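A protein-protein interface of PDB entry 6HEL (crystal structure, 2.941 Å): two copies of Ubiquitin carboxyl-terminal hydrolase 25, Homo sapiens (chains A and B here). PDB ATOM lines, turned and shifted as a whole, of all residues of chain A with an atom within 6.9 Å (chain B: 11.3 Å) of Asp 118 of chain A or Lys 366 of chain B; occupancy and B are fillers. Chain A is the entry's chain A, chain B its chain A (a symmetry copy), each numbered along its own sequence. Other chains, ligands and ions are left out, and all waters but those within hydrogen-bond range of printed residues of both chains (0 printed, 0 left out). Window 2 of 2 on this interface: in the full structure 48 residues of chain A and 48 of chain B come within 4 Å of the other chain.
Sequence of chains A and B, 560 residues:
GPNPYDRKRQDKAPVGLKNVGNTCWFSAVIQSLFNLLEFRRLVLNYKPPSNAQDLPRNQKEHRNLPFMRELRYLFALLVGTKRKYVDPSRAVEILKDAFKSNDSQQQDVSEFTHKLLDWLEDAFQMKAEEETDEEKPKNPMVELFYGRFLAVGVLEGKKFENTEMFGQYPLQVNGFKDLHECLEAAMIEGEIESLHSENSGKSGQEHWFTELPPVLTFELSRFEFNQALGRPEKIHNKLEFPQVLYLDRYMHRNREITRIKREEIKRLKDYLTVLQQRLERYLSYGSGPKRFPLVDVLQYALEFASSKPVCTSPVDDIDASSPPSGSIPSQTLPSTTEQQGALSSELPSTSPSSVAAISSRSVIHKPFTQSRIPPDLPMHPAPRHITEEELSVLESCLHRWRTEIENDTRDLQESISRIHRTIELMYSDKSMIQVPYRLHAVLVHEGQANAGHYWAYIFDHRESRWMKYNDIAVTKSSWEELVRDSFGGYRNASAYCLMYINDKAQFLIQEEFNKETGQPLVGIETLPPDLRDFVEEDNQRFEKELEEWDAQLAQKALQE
The side-chain carboxylate of Asp 118 of chain A lies within salt-bridge range of the side-chain amino group of Lys 366 of chain B (3.9 Å). The side-chain carboxylate (OE2) of Glu 121 of chain A is in salt-bridge range of the side-chain amino group (NZ) of Lys 366 of chain B, 3.5 Å away. The side-chain hydroxyl of Tyr 146 of chain A sits at hydrogen-bond distance from the side-chain amino group of Lys 366 of chain B (3.2 Å). The backbone carbonyl oxygen of Gly 167 of chain A lies close to the backbone NH of His 365 of chain B, 3.3 Å away. The side-chain amide oxygen of Gln 168 of chain A lies close to the backbone carbonyl oxygen of Lys 366 of chain B (2.8 Å). OE1 of Gln 168 of chain A lies close to O of Pro 367 of chain B (2.9 Å). The side-chain amide oxygen (OE1) of Gln 168 of chain A sits at hydrogen-bond distance from the backbone NH (N) of Phe 368 of chain B, at 3.3 Å. The side-chain amide oxygen (OE1) of Gln 168 of chain A is in hydrogen-bond range of the backbone NH (N) of Thr 369 of chain B (3.0 Å).
The backbone carbonyl oxygen (O) of Leu 117 of chain A lies close to the side-chain carboxylate (OE2) of Glu 121 of chain A, 2.5 Å away. The backbone NH of Asp 118 of chain A sits close to the side-chain carboxylate of Glu 121 of chain A (3.2 Å). The side-chain hydroxyl (OH) of Tyr 146 of chain A lies within hydrogen-bond range of the side-chain carboxylate (OE1) of Glu 121 of chain A, 2.8 Å away. The backbone NH (N) of Tyr 169 of chain A sits at hydrogen-bond distance from the backbone carbonyl oxygen (O) of Thr 217 of chain A (2.9 Å). N of Glu 219 of chain A sits at hydrogen-bond distance from O of Tyr 169 of chain A (2.9 Å). The backbone carbonyl oxygen (O) of Lys 366 of chain B sits at hydrogen-bond distance from the side-chain hydroxyl (OG1) of Thr 369 of chain B, 2.9 Å away.
Ser 110 of chain A touches Thr 369 of chain B. Gln 370 of chain B touches Ser 110 of chain A (O to CB, 3.1 Å). Thr 113 of chain A touches Phe 368 of chain B (OG1 to O, 3.6 Å). Thr 369 of chain B touches Thr 113 of chain A (CA to OG1, 3.7 Å). CB of His 114 of chain A touches CG2 of Thr 369 of chain B, 3.3 Å away. Leu 117 of chain A touches Lys 366 of chain B (CB to CG, 3.5 Å). Leu 117 of chain A touches Pro 367 of chain B. Tyr 146 of chain A touches Pro 367 of chain B (OH to CD, 3.8 Å). His 365 of chain B touches Gln 168 of chain A (CB to O, 3.4 Å). CB of Thr 217 of chain A touches O of Pro 367 of chain B (3.6 Å).
Printed residues of chain B within 4 Å of Ser 110 of chain A: Thr 369 (3.1 Å) and Gln 370 (3.1 Å). His 114 of chain A touches just these residues of chain B: Lys 366 (3.3 Å) and Thr 369 (3.3 Å). No residue of chain B comes within 4 Å of Lys 115 of chain A. No residue of chain B comes within 4 Å of Leu 116 of chain A. Asp 118 of chain A touches one residue of chain B. No residue of chain B comes within 4 Å of Leu 120 of chain A. No residue of chain B comes within 4 Å of Asp 122 of chain A. Of chain B, only His 365 comes within 4 Å of Gly 167 of chain A. Of the printed residues of chain B, Gln 168 of chain A touches His 365 (3.4 Å), Lys 366 (2.8 Å), Pro 367 (2.9 Å), Phe 368 (3.3 Å) and Thr 369 (3.0 Å). Of chain A, only His 114, Leu 117, Asp 118, Glu 121, Tyr 146 and Gln 168 come within 4 Å of Lys 366 of chain B. Of the printed residues of chain A, Gln 370 of chain B touches Ser 110. The nearest residue of chain B that does not touch Asp 118 of chain A is Pro 367 of chain B (6.9 Å). The nearest residue of chain A that does not touch Lys 366 of chain B is Gly 167 of chain A (4.5 Å).
Of the 21 printed residues of chain A, 11 touch a printed residue of chain B. Printed residues of chain A that touch a printed residue of chain B: Ser 110, Thr 113, His 114, Leu 117, Asp 118, Glu 121, Tyr 146, Gly 167, Gln 168, Thr 217 and Glu 219. Hydrophobic or aromatic side chains of chain A within 4 Å of the printed part of chain B: His 114, Leu 117 and Tyr 146. Hydrophobic or aromatic side chains of chain B that line the printed part of chain A: His 365, Pro 367 and Phe 368. Along chain B the printed residues that touch a printed residue of chain A span positions 365 to 371. Among the printed residues, Asp or Glu carboxylates within 4 Å of a Lys or Arg side-chain nitrogen of the other chain: Asp 118 of chain A with Lys 366 of chain B and Glu 121 of chain A with Lys 366 of chain B.
No position is printed for both chains. Of the 21 pairs that touch across the chains among the printed residues, none has its exchanged pair printed and touching as well.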
ATOM      1  N   ASN A  64     -24.349 -18.329   5.187  1.00  0.00           N
ATOM      2  CA  ASN A  64     -24.527 -17.145   4.357  1.00  0.00           C
ATOM      3  C   ASN A  64     -24.355 -17.478   2.883  1.00  0.00           C
ATOM      4  O   ASN A  64     -24.999 -16.865   2.033  1.00  0.00           O
ATOM      5  CB  ASN A  64     -23.546 -16.049   4.763  1.00  0.00           C
ATOM      6  CG  ASN A  64     -22.864 -16.336   6.075  1.00  0.00           C
ATOM      7  OD1 ASN A  64     -23.248 -17.243   6.809  1.00  0.00           O
ATOM      8  ND2 ASN A  64     -21.841 -15.551   6.382  1.00  0.00           N
ATOM      9  N   SER A 110     -37.641  -7.440  13.396  1.00  0.00           N
ATOM     10  CA  SER A 110     -36.434  -6.625  13.477  1.00  0.00           C
ATOM     11  C   SER A 110     -35.192  -7.490  13.406  1.00  0.00           C
ATOM     12  O   SER A 110     -34.244  -7.182  12.691  1.00  0.00           O
ATOM     13  CB  SER A 110     -36.426  -5.799  14.765  1.00  0.00           C
ATOM     14  N   THR A 113     -34.807  -9.033   9.977  1.00  0.00           N
ATOM     15  CA  THR A 113     -34.136  -8.095   9.083  1.00  0.00           C
ATOM     16  C   THR A 113     -32.642  -8.022   9.379  1.00  0.00           C
ATOM     17  O   THR A 113     -31.822  -7.916   8.459  1.00  0.00           O
ATOM     18  CB  THR A 113     -34.776  -6.712   9.212  1.00  0.00           C
ATOM     19  OG1 THR A 113     -35.076  -6.459  10.594  1.00  0.00           O
ATOM     20  CG2 THR A 113     -36.060  -6.636   8.405  1.00  0.00           C
ATOM     21  N   HIS A 114     -32.274  -8.098  10.662  1.00  0.00           N
ATOM     22  CA  HIS A 114     -30.872  -8.016  11.068  1.00  0.00           C
ATOM     23  C   HIS A 114     -30.054  -9.165  10.505  1.00  0.00           C
ATOM     24  O   HIS A 114     -28.889  -8.982  10.134  1.00  0.00           O
ATOM     25  CB  HIS A 114     -30.771  -8.018  12.595  1.00  0.00           C
ATOM     26  CG  HIS A 114     -29.409  -8.357  13.113  1.00  0.00           C
ATOM     27  ND1 HIS A 114     -29.059  -9.628  13.511  1.00  0.00           N
ATOM     28  CD2 HIS A 114     -28.313  -7.590  13.313  1.00  0.00           C
ATOM     29  CE1 HIS A 114     -27.805  -9.630  13.926  1.00  0.00           C
ATOM     30  NE2 HIS A 114     -27.328  -8.404  13.813  1.00  0.00           N
ATOM     31  N   LYS A 115     -30.635 -10.364  10.485  1.00  0.00           N
ATOM     32  CA  LYS A 115     -29.885 -11.558  10.117  1.00  0.00           C
ATOM     33  C   LYS A 115     -29.442 -11.505   8.664  1.00  0.00           C
ATOM     34  O   LYS A 115     -28.320 -11.907   8.337  1.00  0.00           O
ATOM     35  CB  LYS A 115     -30.729 -12.804  10.368  1.00  0.00           C
ATOM     36  N   LEU A 116     -30.312 -11.019   7.776  1.00  0.00           N
ATOM     37  CA  LEU A 116     -29.923 -10.862   6.376  1.00  0.00           C
ATOM     38  C   LEU A 116     -28.753  -9.893   6.243  1.00  0.00           C
ATOM     39  O   LEU A 116     -27.751 -10.193   5.584  1.00  0.00           O
ATOM     40  CB  LEU A 116     -31.116 -10.378   5.546  1.00  0.00           C
ATOM     41  N   LEU A 117     -28.870  -8.709   6.838  1.00  0.00           N
ATOM     42  CA  LEU A 117     -27.744  -7.786   6.816  1.00  0.00           C
ATOM     43  C   LEU A 117     -26.472  -8.489   7.293  1.00  0.00           C
ATOM     44  O   LEU A 117     -25.528  -8.667   6.511  1.00  0.00           O
ATOM     45  CB  LEU A 117     -28.114  -6.558   7.647  1.00  0.00           C
ATOM     46  CG  LEU A 117     -29.331  -5.969   6.918  1.00  0.00           C
ATOM     47  CD1 LEU A 117     -29.984  -4.793   7.646  1.00  0.00           C
ATOM     48  CD2 LEU A 117     -28.976  -5.577   5.466  1.00  0.00           C
ATOM     49  N   ASP A 118     -26.513  -9.048   8.508  1.00  0.00           N
ATOM     50  CA  ASP A 118     -25.352  -9.688   9.130  1.00  0.00           C
ATOM     51  C   ASP A 118     -24.711 -10.729   8.211  1.00  0.00           C
ATOM     52  O   ASP A 118     -23.489 -10.724   8.004  1.00  0.00           O
ATOM     53  CB  ASP A 118     -25.759 -10.318  10.467  1.00  0.00           C
ATOM     54  CG  ASP A 118     -24.603 -10.389  11.458  1.00  0.00           C
ATOM     55  OD1 ASP A 118     -23.832  -9.415  11.555  1.00  0.00           O
ATOM     56  OD2 ASP A 118     -24.470 -11.413  12.162  1.00  0.00           O
ATOM     57  N   TRP A 119     -25.522 -11.640   7.664  1.00  0.00           N
ATOM     58  CA  TRP A 119     -25.010 -12.604   6.696  1.00  0.00           C
ATOM     59  C   TRP A 119     -24.328 -11.903   5.534  1.00  0.00           C
ATOM     60  O   TRP A 119     -23.244 -12.312   5.105  1.00  0.00           O
ATOM     61  CB  TRP A 119     -26.139 -13.493   6.176  1.00  0.00           C
ATOM     62  CG  TRP A 119     -26.650 -14.465   7.173  1.00  0.00           C
ATOM     63  CD1 TRP A 119     -26.212 -14.627   8.452  1.00  0.00           C
ATOM     64  CD2 TRP A 119     -27.703 -15.419   6.983  1.00  0.00           C
ATOM     65  NE1 TRP A 119     -26.925 -15.622   9.073  1.00  0.00           N
ATOM     66  CE2 TRP A 119     -27.847 -16.124   8.193  1.00  0.00           C
ATOM     67  CE3 TRP A 119     -28.537 -15.744   5.908  1.00  0.00           C
ATOM     68  CZ2 TRP A 119     -28.789 -17.135   8.360  1.00  0.00           C
ATOM     69  CZ3 TRP A 119     -29.473 -16.748   6.078  1.00  0.00           C
ATOM     70  CH2 TRP A 119     -29.591 -17.432   7.292  1.00  0.00           C
ATOM     71  N   LEU A 120     -24.937 -10.835   5.023  1.00  0.00           N
ATOM     72  CA  LEU A 120     -24.389 -10.179   3.842  1.00  0.00           C
ATOM     73  C   LEU A 120     -23.026  -9.549   4.124  1.00  0.00           C
ATOM     74  O   LEU A 120     -22.071  -9.783   3.375  1.00  0.00           O
ATOM     75  CB  LEU A 120     -25.375  -9.143   3.300  1.00  0.00           C
ATOM     76  CG  LEU A 120     -26.720  -9.642   2.754  1.00  0.00           C
ATOM     77  CD1 LEU A 120     -27.251  -8.700   1.682  1.00  0.00           C
ATOM     78  CD2 LEU A 120     -26.650 -11.072   2.235  1.00  0.00           C
ATOM     79  N   GLU A 121     -22.903  -8.730   5.182  1.00  0.00           N
ATOM     80  CA  GLU A 121     -21.590  -8.093   5.341  1.00  0.00           C
ATOM     81  C   GLU A 121     -20.561  -9.030   5.970  1.00  0.00           C
ATOM     82  O   GLU A 121     -19.370  -8.827   5.737  1.00  0.00           O
ATOM     83  CB  GLU A 121     -21.628  -6.718   6.068  1.00  0.00           C
ATOM     84  CG  GLU A 121     -21.678  -6.632   7.578  1.00  0.00           C
ATOM     85  CD  GLU A 121     -23.045  -6.858   8.069  1.00  0.00           C
ATOM     86  OE1 GLU A 121     -23.653  -5.932   8.646  1.00  0.00           O
ATOM     87  OE2 GLU A 121     -23.537  -7.952   7.846  1.00  0.00           O
ATOM     88  N   ASP A 122     -20.968 -10.129   6.618  1.00  0.00           N
ATOM     89  CA  ASP A 122     -19.983 -11.161   6.944  1.00  0.00           C
ATOM     90  C   ASP A 122     -19.478 -11.865   5.685  1.00  0.00           C
ATOM     91  O   ASP A 122     -18.274 -12.127   5.551  1.00  0.00           O
ATOM     92  CB  ASP A 122     -20.572 -12.175   7.928  1.00  0.00           C
ATOM     93  CG  ASP A 122     -20.558 -11.676   9.360  1.00  0.00           C
ATOM     94  OD1 ASP A 122     -19.699 -10.831   9.695  1.00  0.00           O
ATOM     95  OD2 ASP A 122     -21.405 -12.132  10.154  1.00  0.00           O
ATOM     96  N   ALA A 123     -20.377 -12.163   4.741  1.00  0.00           N
ATOM     97  CA  ALA A 123     -19.965 -12.806   3.498  1.00  0.00           C
ATOM     98  C   ALA A 123     -19.050 -11.898   2.686  1.00  0.00           C
ATOM     99  O   ALA A 123     -18.019 -12.342   2.166  1.00  0.00           O
ATOM    100  CB  ALA A 123     -21.194 -13.206   2.683  1.00  0.00           C
ATOM    101  N   PHE A 124     -19.412 -10.618   2.566  1.00  0.00           N
ATOM    102  CA  PHE A 124     -18.547  -9.672   1.865  1.00  0.00           C
ATOM    103  C   PHE A 124     -17.248  -9.436   2.626  1.00  0.00           C
ATOM    104  O   PHE A 124     -16.224  -9.105   2.016  1.00  0.00           O
ATOM    105  CB  PHE A 124     -19.280  -8.348   1.631  1.00  0.00           C
ATOM    106  CG  PHE A 124     -20.278  -8.391   0.501  1.00  0.00           C
ATOM    107  CD1 PHE A 124     -21.624  -8.581   0.750  1.00  0.00           C
ATOM    108  CD2 PHE A 124     -19.867  -8.231  -0.811  1.00  0.00           C
ATOM    109  CE1 PHE A 124     -22.543  -8.618  -0.278  1.00  0.00           C
ATOM    110  CE2 PHE A 124     -20.783  -8.267  -1.847  1.00  0.00           C
ATOM    111  CZ  PHE A 124     -22.122  -8.462  -1.579  1.00  0.00           C
ATOM    112  N   MET A 141     -19.355  -2.970   2.055  1.00  0.00           N
ATOM    113  CA  MET A 141     -20.590  -2.732   2.769  1.00  0.00           C
ATOM    114  C   MET A 141     -20.413  -1.769   3.921  1.00  0.00           C
ATOM    115  O   MET A 141     -21.084  -0.748   3.987  1.00  0.00           O
ATOM    116  CB  MET A 141     -21.150  -4.048   3.287  1.00  0.00           C
ATOM    117  CG  MET A 141     -21.989  -4.790   2.271  1.00  0.00           C
ATOM    118  SD  MET A 141     -23.735  -4.623   2.651  1.00  0.00           S
ATOM    119  CE  MET A 141     -23.915  -5.843   3.943  1.00  0.00           C
ATOM    120  N   TYR A 146     -22.090   2.399   7.177  1.00  0.00           N
ATOM    121  CA  TYR A 146     -21.643   2.763   8.512  1.00  0.00           C
ATOM    122  C   TYR A 146     -20.599   3.864   8.413  1.00  0.00           C
ATOM    123  O   TYR A 146     -20.016   4.109   7.354  1.00  0.00           O
ATOM    124  CB  TYR A 146     -21.044   1.567   9.273  1.00  0.00           C
ATOM    125  CG  TYR A 146     -21.856   0.289   9.230  1.00  0.00           C
ATOM    126  CD1 TYR A 146     -21.876  -0.504   8.093  1.00  0.00           C
ATOM    127  CD2 TYR A 146     -22.567  -0.145  10.337  1.00  0.00           C
ATOM    128  CE1 TYR A 146     -22.602  -1.675   8.048  1.00  0.00           C
ATOM    129  CE2 TYR A 146     -23.300  -1.317  10.303  1.00  0.00           C
ATOM    130  CZ  TYR A 146     -23.311  -2.079   9.156  1.00  0.00           C
ATOM    131  OH  TYR A 146     -24.035  -3.247   9.113  1.00  0.00           O
ATOM    132  N   GLY A 167     -24.152   2.276  12.571  1.00  0.00           N
ATOM    133  CA  GLY A 167     -24.982   1.849  11.456  1.00  0.00           C
ATOM    134  C   GLY A 167     -26.446   2.154  11.711  1.00  0.00           C
ATOM    135  O   GLY A 167     -26.946   1.849  12.797  1.00  0.00           O
ATOM    136  N   GLN A 168     -27.133   2.781  10.749  1.00  0.00           N
ATOM    137  CA  GLN A 168     -28.555   3.108  10.869  1.00  0.00           C
ATOM    138  C   GLN A 168     -28.869   3.833  12.174  1.00  0.00           C
ATOM    139  O   GLN A 168     -29.361   3.219  13.126  1.00  0.00           O
ATOM    140  CB  GLN A 168     -29.421   1.847  10.771  1.00  0.00           C
ATOM    141  CG  GLN A 168     -30.932   2.114  10.649  1.00  0.00           C
ATOM    142  CD  GLN A 168     -31.779   1.125  11.450  1.00  0.00           C
ATOM    143  OE1 GLN A 168     -32.481   0.291  10.882  1.00  0.00           O
ATOM    144  NE2 GLN A 168     -31.703   1.210  12.774  1.00  0.00           N
ATOM    145  N   TYR A 169     -28.594   5.129  12.224  1.00  0.00           N
ATOM    146  CA  TYR A 169     -28.802   5.906  13.440  1.00  0.00           C
ATOM    147  C   TYR A 169     -30.265   5.839  13.880  1.00  0.00           C
ATOM    148  O   TYR A 169     -31.159   6.123  13.075  1.00  0.00           O
ATOM    149  CB  TYR A 169     -28.382   7.352  13.179  1.00  0.00           C
ATOM    150  CG  TYR A 169     -27.979   8.161  14.388  1.00  0.00           C
ATOM    151  CD1 TYR A 169     -28.035   7.631  15.664  1.00  0.00           C
ATOM    152  CD2 TYR A 169     -27.543   9.471  14.244  1.00  0.00           C
ATOM    153  CE1 TYR A 169     -27.669   8.378  16.766  1.00  0.00           C
ATOM    154  CE2 TYR A 169     -27.175  10.226  15.335  1.00  0.00           C
ATOM    155  CZ  TYR A 169     -27.240   9.677  16.594  1.00  0.00           C
ATOM    156  OH  TYR A 169     -26.872  10.434  17.684  1.00  0.00           O
ATOM    157  N   THR A 217     -28.905   5.586   6.880  1.00  0.00           N
ATOM    158  CA  THR A 217     -30.187   5.006   7.254  1.00  0.00           C
ATOM    159  C   THR A 217     -30.590   5.500   8.635  1.00  0.00           C
ATOM    160  O   THR A 217     -29.878   5.270   9.618  1.00  0.00           O
ATOM    161  CB  THR A 217     -30.128   3.480   7.213  1.00  0.00           C
ATOM    162  OG1 THR A 217     -28.841   3.037   7.657  1.00  0.00           O
ATOM    163  CG2 THR A 217     -30.366   2.983   5.797  1.00  0.00           C
ATOM    164  N   GLU A 219     -33.505   5.283  11.551  1.00  0.00           N
ATOM    165  CA  GLU A 219     -34.658   4.579  12.089  1.00  0.00           C
ATOM    166  C   GLU A 219     -35.564   5.573  12.798  1.00  0.00           C
ATOM    167  O   GLU A 219     -35.090   6.439  13.533  1.00  0.00           O
ATOM    168  CB  GLU A 219     -34.222   3.482  13.062  1.00  0.00           C
ATOM    169  N   SER B 362     -22.291   1.897  22.290  1.00  0.00           N
ATOM    170  CA  SER B 362     -23.651   1.923  21.771  1.00  0.00           C
ATOM    171  C   SER B 362     -23.862   0.713  20.877  1.00  0.00           C
ATOM    172  O   SER B 362     -23.036   0.431  20.004  1.00  0.00           O
ATOM    173  CB  SER B 362     -23.921   3.214  20.985  1.00  0.00           C
ATOM    174  OG  SER B 362     -23.776   4.353  21.814  1.00  0.00           O
ATOM    175  N   VAL B 363     -24.959  -0.006  21.103  1.00  0.00           N
ATOM    176  CA  VAL B 363     -25.292  -1.171  20.293  1.00  0.00           C
ATOM    177  C   VAL B 363     -25.526  -0.721  18.857  1.00  0.00           C
ATOM    178  O   VAL B 363     -26.597  -0.195  18.532  1.00  0.00           O
ATOM    179  CB  VAL B 363     -26.524  -1.904  20.854  1.00  0.00           C
ATOM    180  N   ILE B 364     -24.523  -0.916  17.993  1.00  0.00           N
ATOM    181  CA  ILE B 364     -24.640  -0.488  16.606  1.00  0.00           C
ATOM    182  C   ILE B 364     -25.841  -1.166  15.968  1.00  0.00           C
ATOM    183  O   ILE B 364     -26.130  -2.342  16.226  1.00  0.00           O
ATOM    184  CB  ILE B 364     -23.343  -0.782  15.834  1.00  0.00           C
ATOM    185  CG1 ILE B 364     -22.934  -2.249  16.003  1.00  0.00           C
ATOM    186  CG2 ILE B 364     -22.231   0.144  16.295  1.00  0.00           C
ATOM    187  CD1 ILE B 364     -23.318  -3.137  14.831  1.00  0.00           C
ATOM    188  N   HIS B 365     -26.563  -0.417  15.144  1.00  0.00           N
ATOM    189  CA  HIS B 365     -27.824  -0.885  14.590  1.00  0.00           C
ATOM    190  C   HIS B 365     -27.653  -1.366  13.153  1.00  0.00           C
ATOM    191  O   HIS B 365     -26.887  -0.789  12.373  1.00  0.00           O
ATOM    192  CB  HIS B 365     -28.882   0.213  14.649  1.00  0.00           C
ATOM    193  CG  HIS B 365     -29.820   0.067  15.805  1.00  0.00           C
ATOM    194  ND1 HIS B 365     -29.694   0.794  16.970  1.00  0.00           N
ATOM    195  CD2 HIS B 365     -30.895  -0.737  15.979  1.00  0.00           C
ATOM    196  CE1 HIS B 365     -30.659   0.450  17.808  1.00  0.00           C
ATOM    197  NE2 HIS B 365     -31.398  -0.479  17.231  1.00  0.00           N
ATOM    198  N   LYS B 366     -28.366  -2.435  12.809  1.00  0.00           N
ATOM    199  CA  LYS B 366     -28.423  -2.859  11.421  1.00  0.00           C
ATOM    200  C   LYS B 366     -29.245  -1.873  10.600  1.00  0.00           C
ATOM    201  O   LYS B 366     -30.141  -1.219  11.130  1.00  0.00           O
ATOM    202  CB  LYS B 366     -29.011  -4.258  11.296  1.00  0.00           C
ATOM    203  CG  LYS B 366     -27.981  -5.275  10.936  1.00  0.00           C
ATOM    204  CD  LYS B 366     -26.777  -5.111  11.848  1.00  0.00           C
ATOM    205  CE  LYS B 366     -25.794  -6.208  11.590  1.00  0.00           C
ATOM    206  NZ  LYS B 366     -25.246  -6.047  10.222  1.00  0.00           N
ATOM    207  N   PRO B 367     -28.938  -1.747   9.303  1.00  0.00           N
ATOM    208  CA  PRO B 367     -29.557  -0.681   8.487  1.00  0.00           C
ATOM    209  C   PRO B 367     -31.078  -0.704   8.394  1.00  0.00           C
ATOM    210  O   PRO B 367     -31.678   0.348   8.133  1.00  0.00           O
ATOM    211  CB  PRO B 367     -28.924  -0.894   7.108  1.00  0.00           C
ATOM    212  CG  PRO B 367     -27.614  -1.536   7.377  1.00  0.00           C
ATOM    213  CD  PRO B 367     -27.727  -2.303   8.670  1.00  0.00           C
ATOM    214  N   PHE B 368     -31.726  -1.860   8.549  1.00  0.00           N
ATOM    215  CA  PHE B 368     -33.172  -1.942   8.370  1.00  0.00           C
ATOM    216  C   PHE B 368     -33.862  -2.585   9.566  1.00  0.00           C
ATOM    217  O   PHE B 368     -35.005  -3.037   9.450  1.00  0.00           O
ATOM    218  CB  PHE B 368     -33.504  -2.694   7.080  1.00  0.00           C
ATOM    219  CG  PHE B 368     -33.039  -1.986   5.842  1.00  0.00           C
ATOM    220  CD1 PHE B 368     -33.914  -1.213   5.098  1.00  0.00           C
ATOM    221  CD2 PHE B 368     -31.720  -2.074   5.431  1.00  0.00           C
ATOM    222  CE1 PHE B 368     -33.480  -0.551   3.966  1.00  0.00           C
ATOM    223  CE2 PHE B 368     -31.285  -1.412   4.305  1.00  0.00           C
ATOM    224  CZ  PHE B 368     -32.164  -0.653   3.572  1.00  0.00           C
ATOM    225  N   THR B 369     -33.202  -2.619  10.718  1.00  0.00           N
ATOM    226  CA  THR B 369     -33.782  -3.263  11.885  1.00  0.00           C
ATOM    227  C   THR B 369     -34.683  -2.316  12.652  1.00  0.00           C
ATOM    228  O   THR B 369     -34.302  -1.185  12.972  1.00  0.00           O
ATOM    229  CB  THR B 369     -32.705  -3.785  12.826  1.00  0.00           C
ATOM    230  OG1 THR B 369     -31.698  -2.785  13.009  1.00  0.00           O
ATOM    231  CG2 THR B 369     -32.103  -5.003  12.261  1.00  0.00           C
ATOM    232  N   GLN B 370     -35.878  -2.799  12.955  1.00  0.00           N
ATOM    233  CA  GLN B 370     -36.720  -2.155  13.942  1.00  0.00           C
ATOM    234  C   GLN B 370     -35.993  -2.103  15.280  1.00  0.00           C
ATOM    235  O   GLN B 370     -35.370  -3.077  15.708  1.00  0.00           O
ATOM    236  CB  GLN B 370     -38.025  -2.927  14.072  1.00  0.00           C
ATOM    237  CG  GLN B 370     -38.917  -2.856  12.856  1.00  0.00           C
ATOM    238  CD  GLN B 370     -39.966  -1.777  12.995  1.00  0.00           C
ATOM    239  OE1 GLN B 370     -39.692  -0.695  13.511  1.00  0.00           O
ATOM    240  NE2 GLN B 370     -41.184  -2.074  12.554  1.00  0.00           N
ATOM    241  N   SER B 371     -36.062  -0.957  15.937  1.00  0.00           N
ATOM    242  CA  SER B 371     -35.420  -0.770  17.225  1.00  0.00           C
ATOM    243  C   SER B 371     -36.479  -0.589  18.299  1.00  0.00           C
ATOM    244  O   SER B 371     -37.489   0.084  18.079  1.00  0.00           O
ATOM    245  CB  SER B 371     -34.483   0.437  17.193  1.00  0.00           C
ATOM    246  OG  SER B 371     -35.011   1.462  16.370  1.00  0.00           O
ATOM    247  N   ARG B 372     -36.248  -1.206  19.460  1.00  0.00           N
ATOM    248  CA  ARG B 372     -37.110  -1.020  20.625  1.00  0.00           C
ATOM    249  C   ARG B 372     -38.544  -1.443  20.315  1.00  0.00           C
ATOM    250  O   ARG B 372     -39.514  -0.759  20.651  1.00  0.00           O
ATOM    251  CB  ARG B 372     -37.052   0.433  21.103  1.00  0.00           C
ATOM    252  CG  ARG B 372     -37.747   0.733  22.417  1.00  0.00           C
ATOM    253  CD  ARG B 372     -38.235   2.163  22.383  1.00  0.00           C
ATOM    254  NE  ARG B 372     -37.190   3.041  21.870  1.00  0.00           N
ATOM    255  CZ  ARG B 372     -37.372   4.314  21.540  1.00  0.00           C
ATOM    256  NH1 ARG B 372     -38.569   4.867  21.662  1.00  0.00           N
ATOM    257  NH2 ARG B 372     -36.353   5.028  21.083  1.00  0.00           N
